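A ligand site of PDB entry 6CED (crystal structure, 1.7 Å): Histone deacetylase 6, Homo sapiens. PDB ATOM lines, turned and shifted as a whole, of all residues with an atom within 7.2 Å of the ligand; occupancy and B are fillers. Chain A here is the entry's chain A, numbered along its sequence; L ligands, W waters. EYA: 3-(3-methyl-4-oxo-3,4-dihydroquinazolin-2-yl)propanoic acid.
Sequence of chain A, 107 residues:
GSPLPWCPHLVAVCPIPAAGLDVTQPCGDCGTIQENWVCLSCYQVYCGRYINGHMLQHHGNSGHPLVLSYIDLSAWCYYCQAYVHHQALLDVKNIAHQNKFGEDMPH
O of the ligand is in hydrogen-bond range of N of Arg 49 (2.9 Å). The guanidinium group (NH2) of Arg 49 lies within salt-bridge range of an oxygen (O) of the ligand. The side-chain hydroxyl (OH) of Tyr 78 lies within hydrogen-bond range of an oxygen (O1) of the ligand, 2.6 Å away.
O of Tyr 46 lies within hydrogen-bond range of N of Trp 37 (2.9 Å). The backbone carbonyl oxygen of Glu 35 lies within hydrogen-bond range of the backbone NH of Gly 48 (2.8 Å). N of Trp 76 sits at hydrogen-bond distance from O of Val 67. N of Gly 53 sits at hydrogen-bond distance from O of Gly 48, at 3.0 Å.
Residues that only touch the ligand: Tyr 83 (3.2 Å), Trp 76 (3.4 Å), Trp 37 (3.4 Å), Gly 48 (3.6 Å) and Leu 56 (3.98 Å). Hydrophobic or aromatic side chains that line the ligand: Trp 37, Trp 76, Tyr 78 and Tyr 83. Of the 21 residues printed, 7 come within 4 Å of the ligand. The nearest printed residue that does not touch the ligand is Met 55 (4.2 Å).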
ATOM      1  N   GLU A  35      -4.228  -3.846  -5.719  1.00  0.00           N
ATOM      2  CA  GLU A  35      -5.634  -3.543  -5.772  1.00  0.00           C
ATOM      3  C   GLU A  35      -6.488  -4.834  -5.706  1.00  0.00           C
ATOM      4  O   GLU A  35      -7.432  -4.974  -6.441  1.00  0.00           O
ATOM      5  CB  GLU A  35      -6.017  -2.804  -7.051  1.00  0.00           C
ATOM      6  CG  GLU A  35      -5.287  -1.528  -7.368  1.00  0.00           C
ATOM      7  CD  GLU A  35      -6.045  -0.270  -6.902  1.00  0.00           C
ATOM      8  OE1 GLU A  35      -7.216  -0.116  -7.295  1.00  0.00           O
ATOM      9  OE2 GLU A  35      -5.436   0.577  -6.202  1.00  0.00           O
ATOM     10  N   TRP A  37      -9.217  -7.485  -3.938  1.00  0.00           N
ATOM     11  CA  TRP A  37     -10.452  -7.568  -3.195  1.00  0.00           C
ATOM     12  C   TRP A  37     -10.691  -8.989  -2.791  1.00  0.00           C
ATOM     13  O   TRP A  37     -10.211  -9.908  -3.444  1.00  0.00           O
ATOM     14  CB  TRP A  37     -11.607  -7.137  -4.098  1.00  0.00           C
ATOM     15  CG  TRP A  37     -11.543  -5.749  -4.579  1.00  0.00           C
ATOM     16  CD1 TRP A  37     -10.692  -5.263  -5.545  1.00  0.00           C
ATOM     17  CD2 TRP A  37     -12.367  -4.619  -4.189  1.00  0.00           C
ATOM     18  NE1 TRP A  37     -10.887  -3.923  -5.762  1.00  0.00           N
ATOM     19  CE2 TRP A  37     -11.914  -3.489  -4.961  1.00  0.00           C
ATOM     20  CE3 TRP A  37     -13.389  -4.446  -3.297  1.00  0.00           C
ATOM     21  CZ2 TRP A  37     -12.505  -2.226  -4.860  1.00  0.00           C
ATOM     22  CZ3 TRP A  37     -13.987  -3.184  -3.177  1.00  0.00           C
ATOM     23  CH2 TRP A  37     -13.529  -2.094  -3.949  1.00  0.00           C
ATOM     24  N   TYR A  46      -9.264 -11.598  -5.803  1.00  0.00           N
ATOM     25  CA  TYR A  46      -9.045 -11.252  -7.152  1.00  0.00           C
ATOM     26  C   TYR A  46      -8.820  -9.741  -7.298  1.00  0.00           C
ATOM     27  O   TYR A  46      -9.284  -8.954  -6.488  1.00  0.00           O
ATOM     28  CB  TYR A  46     -10.192 -11.670  -8.066  1.00  0.00           C
ATOM     29  CG  TYR A  46     -10.450 -13.147  -8.133  1.00  0.00           C
ATOM     30  CD1 TYR A  46      -9.523 -13.985  -8.775  1.00  0.00           C
ATOM     31  CD2 TYR A  46     -11.555 -13.685  -7.522  1.00  0.00           C
ATOM     32  CE1 TYR A  46      -9.754 -15.322  -8.855  1.00  0.00           C
ATOM     33  CE2 TYR A  46     -11.796 -15.078  -7.577  1.00  0.00           C
ATOM     34  CZ  TYR A  46     -10.876 -15.878  -8.240  1.00  0.00           C
ATOM     35  OH  TYR A  46     -11.058 -17.268  -8.273  1.00  0.00           O
ATOM     36  N   CYS A  47      -8.157  -9.338  -8.372  1.00  0.00           N
ATOM     37  CA  CYS A  47      -7.788  -7.955  -8.537  1.00  0.00           C
ATOM     38  C   CYS A  47      -8.937  -7.049  -9.064  1.00  0.00           C
ATOM     39  O   CYS A  47      -9.883  -7.465  -9.732  1.00  0.00           O
ATOM     40  CB  CYS A  47      -6.518  -7.860  -9.438  1.00  0.00           C
ATOM     41  SG  CYS A  47      -6.805  -8.359 -11.170  1.00  0.00           S
ATOM     42  N   GLY A  48      -8.748  -5.767  -8.790  1.00  0.00           N
ATOM     43  CA  GLY A  48      -9.637  -4.714  -9.167  1.00  0.00           C
ATOM     44  C   GLY A  48      -9.657  -4.332 -10.624  1.00  0.00           C
ATOM     45  O   GLY A  48      -8.820  -4.753 -11.399  1.00  0.00           O
ATOM     46  N   ARG A  49     -10.628  -3.490 -10.950  1.00  0.00           N
ATOM     47  CA  ARG A  49     -10.922  -3.078 -12.304  1.00  0.00           C
ATOM     48  C   ARG A  49      -9.727  -2.435 -12.992  1.00  0.00           C
ATOM     49  O   ARG A  49      -9.480  -2.702 -14.191  1.00  0.00           O
ATOM     50  CB  ARG A  49     -12.121  -2.098 -12.320  1.00  0.00           C
ATOM     51  CG  ARG A  49     -11.936  -0.837 -11.493  1.00  0.00           C
ATOM     52  CD  ARG A  49     -13.267  -0.250 -11.051  1.00  0.00           C
ATOM     53  NE  ARG A  49     -13.197   1.014 -10.288  1.00  0.00           N
ATOM     54  CZ  ARG A  49     -12.732   1.124  -9.049  1.00  0.00           C
ATOM     55  NH1 ARG A  49     -12.712   2.293  -8.407  1.00  0.00           N
ATOM     56  NH2 ARG A  49     -12.288   0.032  -8.444  1.00  0.00           N
ATOM     57  N   TYR A  50      -8.957  -1.681 -12.217  1.00  0.00           N
ATOM     58  CA  TYR A  50      -7.831  -0.922 -12.741  1.00  0.00           C
ATOM     59  C   TYR A  50      -6.590  -1.764 -12.946  1.00  0.00           C
ATOM     60  O   TYR A  50      -5.656  -1.275 -13.603  1.00  0.00           O
ATOM     61  CB  TYR A  50      -7.533   0.348 -11.947  1.00  0.00           C
ATOM     62  CG  TYR A  50      -8.665   1.361 -12.022  1.00  0.00           C
ATOM     63  CD1 TYR A  50      -9.160   1.779 -13.257  1.00  0.00           C
ATOM     64  CD2 TYR A  50      -9.225   1.889 -10.869  1.00  0.00           C
ATOM     65  CE1 TYR A  50     -10.196   2.698 -13.356  1.00  0.00           C
ATOM     66  CE2 TYR A  50     -10.249   2.803 -10.964  1.00  0.00           C
ATOM     67  CZ  TYR A  50     -10.738   3.200 -12.220  1.00  0.00           C
ATOM     68  OH  TYR A  50     -11.767   4.097 -12.371  1.00  0.00           O
ATOM     69  N   ILE A  51      -6.567  -3.012 -12.486  1.00  0.00           N
ATOM     70  CA  ILE A  51      -5.465  -3.934 -12.748  1.00  0.00           C
ATOM     71  C   ILE A  51      -5.921  -4.811 -13.917  1.00  0.00           C
ATOM     72  O   ILE A  51      -5.898  -4.389 -15.089  1.00  0.00           O
ATOM     73  CB  ILE A  51      -5.029  -4.683 -11.450  1.00  0.00           C
ATOM     74  CG1 ILE A  51      -4.733  -3.638 -10.350  1.00  0.00           C
ATOM     75  CG2 ILE A  51      -3.802  -5.545 -11.714  1.00  0.00           C
ATOM     76  CD1 ILE A  51      -3.654  -2.634 -10.673  1.00  0.00           C
ATOM     77  N   GLY A  53      -9.062  -6.688 -13.651  1.00  0.00           N
ATOM     78  CA  GLY A  53     -10.533  -6.894 -13.549  1.00  0.00           C
ATOM     79  C   GLY A  53     -10.958  -8.295 -13.192  1.00  0.00           C
ATOM     80  O   GLY A  53     -12.071  -8.719 -13.548  1.00  0.00           O
ATOM     81  N   HIS A  54     -10.103  -9.057 -12.519  1.00  0.00           N
ATOM     82  CA  HIS A  54     -10.453 -10.441 -12.196  1.00  0.00           C
ATOM     83  C   HIS A  54     -11.593 -10.573 -11.176  1.00  0.00           C
ATOM     84  O   HIS A  54     -12.340 -11.575 -11.253  1.00  0.00           O
ATOM     85  CB  HIS A  54      -9.215 -11.249 -11.823  1.00  0.00           C
ATOM     86  CG  HIS A  54      -8.350 -11.455 -13.011  1.00  0.00           C
ATOM     87  ND1 HIS A  54      -6.993 -11.181 -13.044  1.00  0.00           N
ATOM     88  CD2 HIS A  54      -8.677 -11.920 -14.244  1.00  0.00           C
ATOM     89  CE1 HIS A  54      -6.532 -11.483 -14.251  1.00  0.00           C
ATOM     90  NE2 HIS A  54      -7.537 -11.886 -15.015  1.00  0.00           N
ATOM     91  N   MET A  55     -11.752  -9.593 -10.260  1.00  0.00           N
ATOM     92  CA  MET A  55     -12.878  -9.685  -9.349  1.00  0.00           C
ATOM     93  C   MET A  55     -14.198  -9.424 -10.089  1.00  0.00           C
ATOM     94  O   MET A  55     -15.209 -10.102  -9.795  1.00  0.00           O
ATOM     95  CB  MET A  55     -12.752  -8.781  -8.108  1.00  0.00           C
ATOM     96  CG  MET A  55     -13.843  -9.065  -7.079  1.00  0.00           C
ATOM     97  SD  MET A  55     -13.911 -10.760  -6.491  1.00  0.00           S
ATOM     98  CE  MET A  55     -12.735 -10.688  -5.194  1.00  0.00           C
ATOM     99  N   LEU A  56     -14.181  -8.478 -11.024  1.00  0.00           N
ATOM    100  CA  LEU A  56     -15.359  -8.211 -11.840  1.00  0.00           C
ATOM    101  C   LEU A  56     -15.682  -9.469 -12.643  1.00  0.00           C
ATOM    102  O   LEU A  56     -16.887  -9.837 -12.774  1.00  0.00           O
ATOM    103  CB  LEU A  56     -15.078  -6.988 -12.776  1.00  0.00           C
ATOM    104  CG  LEU A  56     -16.219  -6.640 -13.711  1.00  0.00           C
ATOM    105  CD1 LEU A  56     -17.506  -6.378 -12.975  1.00  0.00           C
ATOM    106  CD2 LEU A  56     -15.815  -5.439 -14.581  1.00  0.00           C
ATOM    107  N   GLN A  57     -14.653 -10.172 -13.163  1.00  0.00           N
ATOM    108  CA  GLN A  57     -14.863 -11.422 -13.881  1.00  0.00           C
ATOM    109  C   GLN A  57     -15.494 -12.493 -12.958  1.00  0.00           C
ATOM    110  O   GLN A  57     -16.441 -13.197 -13.315  1.00  0.00           O
ATOM    111  CB  GLN A  57     -13.582 -11.927 -14.518  1.00  0.00           C
ATOM    112  CG  GLN A  57     -13.716 -13.139 -15.408  1.00  0.00           C
ATOM    113  CD  GLN A  57     -12.362 -13.527 -16.032  1.00  0.00           C
ATOM    114  OE1 GLN A  57     -11.456 -12.714 -16.122  1.00  0.00           O
ATOM    115  NE2 GLN A  57     -12.223 -14.809 -16.430  1.00  0.00           N
ATOM    116  N   VAL A  67     -17.893  -7.461  -2.320  1.00  0.00           N
ATOM    117  CA  VAL A  67     -16.448  -7.665  -2.298  1.00  0.00           C
ATOM    118  C   VAL A  67     -15.855  -6.571  -1.384  1.00  0.00           C
ATOM    119  O   VAL A  67     -16.349  -5.460  -1.365  1.00  0.00           O
ATOM    120  CB  VAL A  67     -15.814  -7.699  -3.700  1.00  0.00           C
ATOM    121  CG1 VAL A  67     -16.343  -8.905  -4.449  1.00  0.00           C
ATOM    122  CG2 VAL A  67     -16.085  -6.405  -4.516  1.00  0.00           C
ATOM    123  N   SER A  74     -13.248  -0.897   2.115  1.00  0.00           N
ATOM    124  CA  SER A  74     -14.592  -0.582   1.636  1.00  0.00           C
ATOM    125  C   SER A  74     -15.236  -1.832   1.046  1.00  0.00           C
ATOM    126  O   SER A  74     -14.542  -2.667   0.521  1.00  0.00           O
ATOM    127  CB  SER A  74     -14.588   0.571   0.657  1.00  0.00           C
ATOM    128  OG  SER A  74     -13.975   0.264  -0.547  1.00  0.00           O
ATOM    129  N   TRP A  76     -17.990  -3.149  -1.841  1.00  0.00           N
ATOM    130  CA  TRP A  76     -18.659  -2.819  -3.041  1.00  0.00           C
ATOM    131  C   TRP A  76     -19.651  -3.897  -3.407  1.00  0.00           C
ATOM    132  O   TRP A  76     -19.336  -5.104  -3.339  1.00  0.00           O
ATOM    133  CB  TRP A  76     -17.679  -2.655  -4.215  1.00  0.00           C
ATOM    134  CG  TRP A  76     -18.253  -2.338  -5.519  1.00  0.00           C
ATOM    135  CD1 TRP A  76     -18.441  -3.197  -6.566  1.00  0.00           C
ATOM    136  CD2 TRP A  76     -18.720  -1.049  -5.959  1.00  0.00           C
ATOM    137  NE1 TRP A  76     -18.967  -2.508  -7.635  1.00  0.00           N
ATOM    138  CE2 TRP A  76     -19.144  -1.193  -7.292  1.00  0.00           C
ATOM    139  CE3 TRP A  76     -18.766   0.198  -5.379  1.00  0.00           C
ATOM    140  CZ2 TRP A  76     -19.665  -0.101  -8.053  1.00  0.00           C
ATOM    141  CZ3 TRP A  76     -19.277   1.284  -6.127  1.00  0.00           C
ATOM    142  CH2 TRP A  76     -19.698   1.120  -7.449  1.00  0.00           C
ATOM    143  N   CYS A  77     -20.867  -3.489  -3.757  1.00  0.00           N
ATOM    144  CA  CYS A  77     -21.806  -4.400  -4.317  1.00  0.00           C
ATOM    145  C   CYS A  77     -21.918  -4.219  -5.822  1.00  0.00           C
ATOM    146  O   CYS A  77     -22.280  -3.129  -6.311  1.00  0.00           O
ATOM    147  CB  CYS A  77     -23.215  -4.220  -3.739  1.00  0.00           C
ATOM    148  SG  CYS A  77     -24.437  -5.375  -4.463  1.00  0.00           S
ATOM    149  N   TYR A  78     -21.660  -5.256  -6.576  1.00  0.00           N
ATOM    150  CA  TYR A  78     -21.648  -5.108  -8.037  1.00  0.00           C
ATOM    151  C   TYR A  78     -23.057  -4.936  -8.635  1.00  0.00           C
ATOM    152  O   TYR A  78     -23.201  -4.368  -9.719  1.00  0.00           O
ATOM    153  CB  TYR A  78     -20.990  -6.317  -8.739  1.00  0.00           C
ATOM    154  CG  TYR A  78     -19.478  -6.421  -8.612  1.00  0.00           C
ATOM    155  CD1 TYR A  78     -18.663  -5.578  -9.375  1.00  0.00           C
ATOM    156  CD2 TYR A  78     -18.860  -7.348  -7.749  1.00  0.00           C
ATOM    157  CE1 TYR A  78     -17.288  -5.663  -9.275  1.00  0.00           C
ATOM    158  CE2 TYR A  78     -17.477  -7.396  -7.623  1.00  0.00           C
ATOM    159  CZ  TYR A  78     -16.709  -6.572  -8.394  1.00  0.00           C
ATOM    160  OH  TYR A  78     -15.363  -6.645  -8.262  1.00  0.00           O
ATOM    161  N   GLN A  81     -24.177  -1.405  -7.606  1.00  0.00           N
ATOM    162  CA  GLN A  81     -23.160  -0.473  -8.127  1.00  0.00           C
ATOM    163  C   GLN A  81     -22.966   0.644  -7.114  1.00  0.00           C
ATOM    164  O   GLN A  81     -22.965   1.859  -7.428  1.00  0.00           O
ATOM    165  CB  GLN A  81     -23.493   0.049  -9.531  1.00  0.00           C
ATOM    166  CG  GLN A  81     -24.040  -0.986 -10.477  1.00  0.00           C
ATOM    167  CD  GLN A  81     -24.513  -0.307 -11.784  1.00  0.00           C
ATOM    168  OE1 GLN A  81     -25.700  -0.070 -11.995  1.00  0.00           O
ATOM    169  NE2 GLN A  81     -23.571   0.065 -12.595  1.00  0.00           N
ATOM    170  N   ALA A  82     -22.710   0.228  -5.892  1.00  0.00           N
ATOM    171  CA  ALA A  82     -22.499   1.143  -4.790  1.00  0.00           C
ATOM    172  C   ALA A  82     -21.685   0.526  -3.706  1.00  0.00           C
ATOM    173  O   ALA A  82     -21.675  -0.700  -3.582  1.00  0.00           O
ATOM    174  CB  ALA A  82     -23.823   1.614  -4.214  1.00  0.00           C
ATOM    175  N   TYR A  83     -21.070   1.394  -2.895  1.00  0.00           N
ATOM    176  CA  TYR A  83     -20.461   0.948  -1.630  1.00  0.00           C
ATOM    177  C   TYR A  83     -21.541   0.776  -0.600  1.00  0.00           C
ATOM    178  O   TYR A  83     -22.562   1.504  -0.620  1.00  0.00           O
ATOM    179  CB  TYR A  83     -19.420   1.957  -1.164  1.00  0.00           C
ATOM    180  CG  TYR A  83     -18.218   1.954  -2.022  1.00  0.00           C
ATOM    181  CD1 TYR A  83     -17.274   0.946  -1.888  1.00  0.00           C
ATOM    182  CD2 TYR A  83     -17.966   3.017  -2.915  1.00  0.00           C
ATOM    183  CE1 TYR A  83     -16.112   0.953  -2.685  1.00  0.00           C
ATOM    184  CE2 TYR A  83     -16.837   2.988  -3.737  1.00  0.00           C
ATOM    185  CZ  TYR A  83     -15.930   2.011  -3.572  1.00  0.00           C
ATOM    186  OH  TYR A  83     -14.826   2.037  -4.389  1.00  0.00           O
HETATM  187  C1  EYA L   1     -15.657  -1.415  -8.415  1.00  0.00           C
HETATM  188  C2  EYA L   1     -14.904  -2.053  -7.301  1.00  0.00           C
HETATM  189  C3  EYA L   1     -14.565  -3.515  -7.573  1.00  0.00           C
HETATM  190  C4  EYA L   1     -13.668  -3.826  -8.757  1.00  0.00           C
HETATM  191  C5  EYA L   1     -16.629  -1.554 -10.497  1.00  0.00           C
HETATM  192  C6  EYA L   1     -16.973  -2.349 -11.597  1.00  0.00           C
HETATM  193  C7  EYA L   1     -17.653  -1.787 -12.668  1.00  0.00           C
HETATM  194  C8  EYA L   1     -18.008  -0.459 -12.646  1.00  0.00           C
HETATM  195  O1  EYA L   1     -13.804  -4.878  -9.381  1.00  0.00           O
HETATM  196  N1  EYA L   1     -15.931  -2.144  -9.443  1.00  0.00           N
HETATM  197  N   EYA L   1     -15.993  -0.073  -8.311  1.00  0.00           N
HETATM  198  C   EYA L   1     -15.661   0.682  -7.110  1.00  0.00           C
HETATM  199  O   EYA L   1     -12.721  -2.909  -8.974  1.00  0.00           O
HETATM  200  O2  EYA L   1     -16.881   1.774  -9.276  1.00  0.00           O
HETATM  201  C11 EYA L   1     -16.653   0.598  -9.345  1.00  0.00           C
HETATM  202  C10 EYA L   1     -16.988  -0.208 -10.486  1.00  0.00           C
HETATM  203  C9  EYA L   1     -17.678   0.339 -11.572  1.00  0.00           C
HETATM  204  O   HOH W   1     -12.208  -6.352 -10.896  1.00  0.00           O
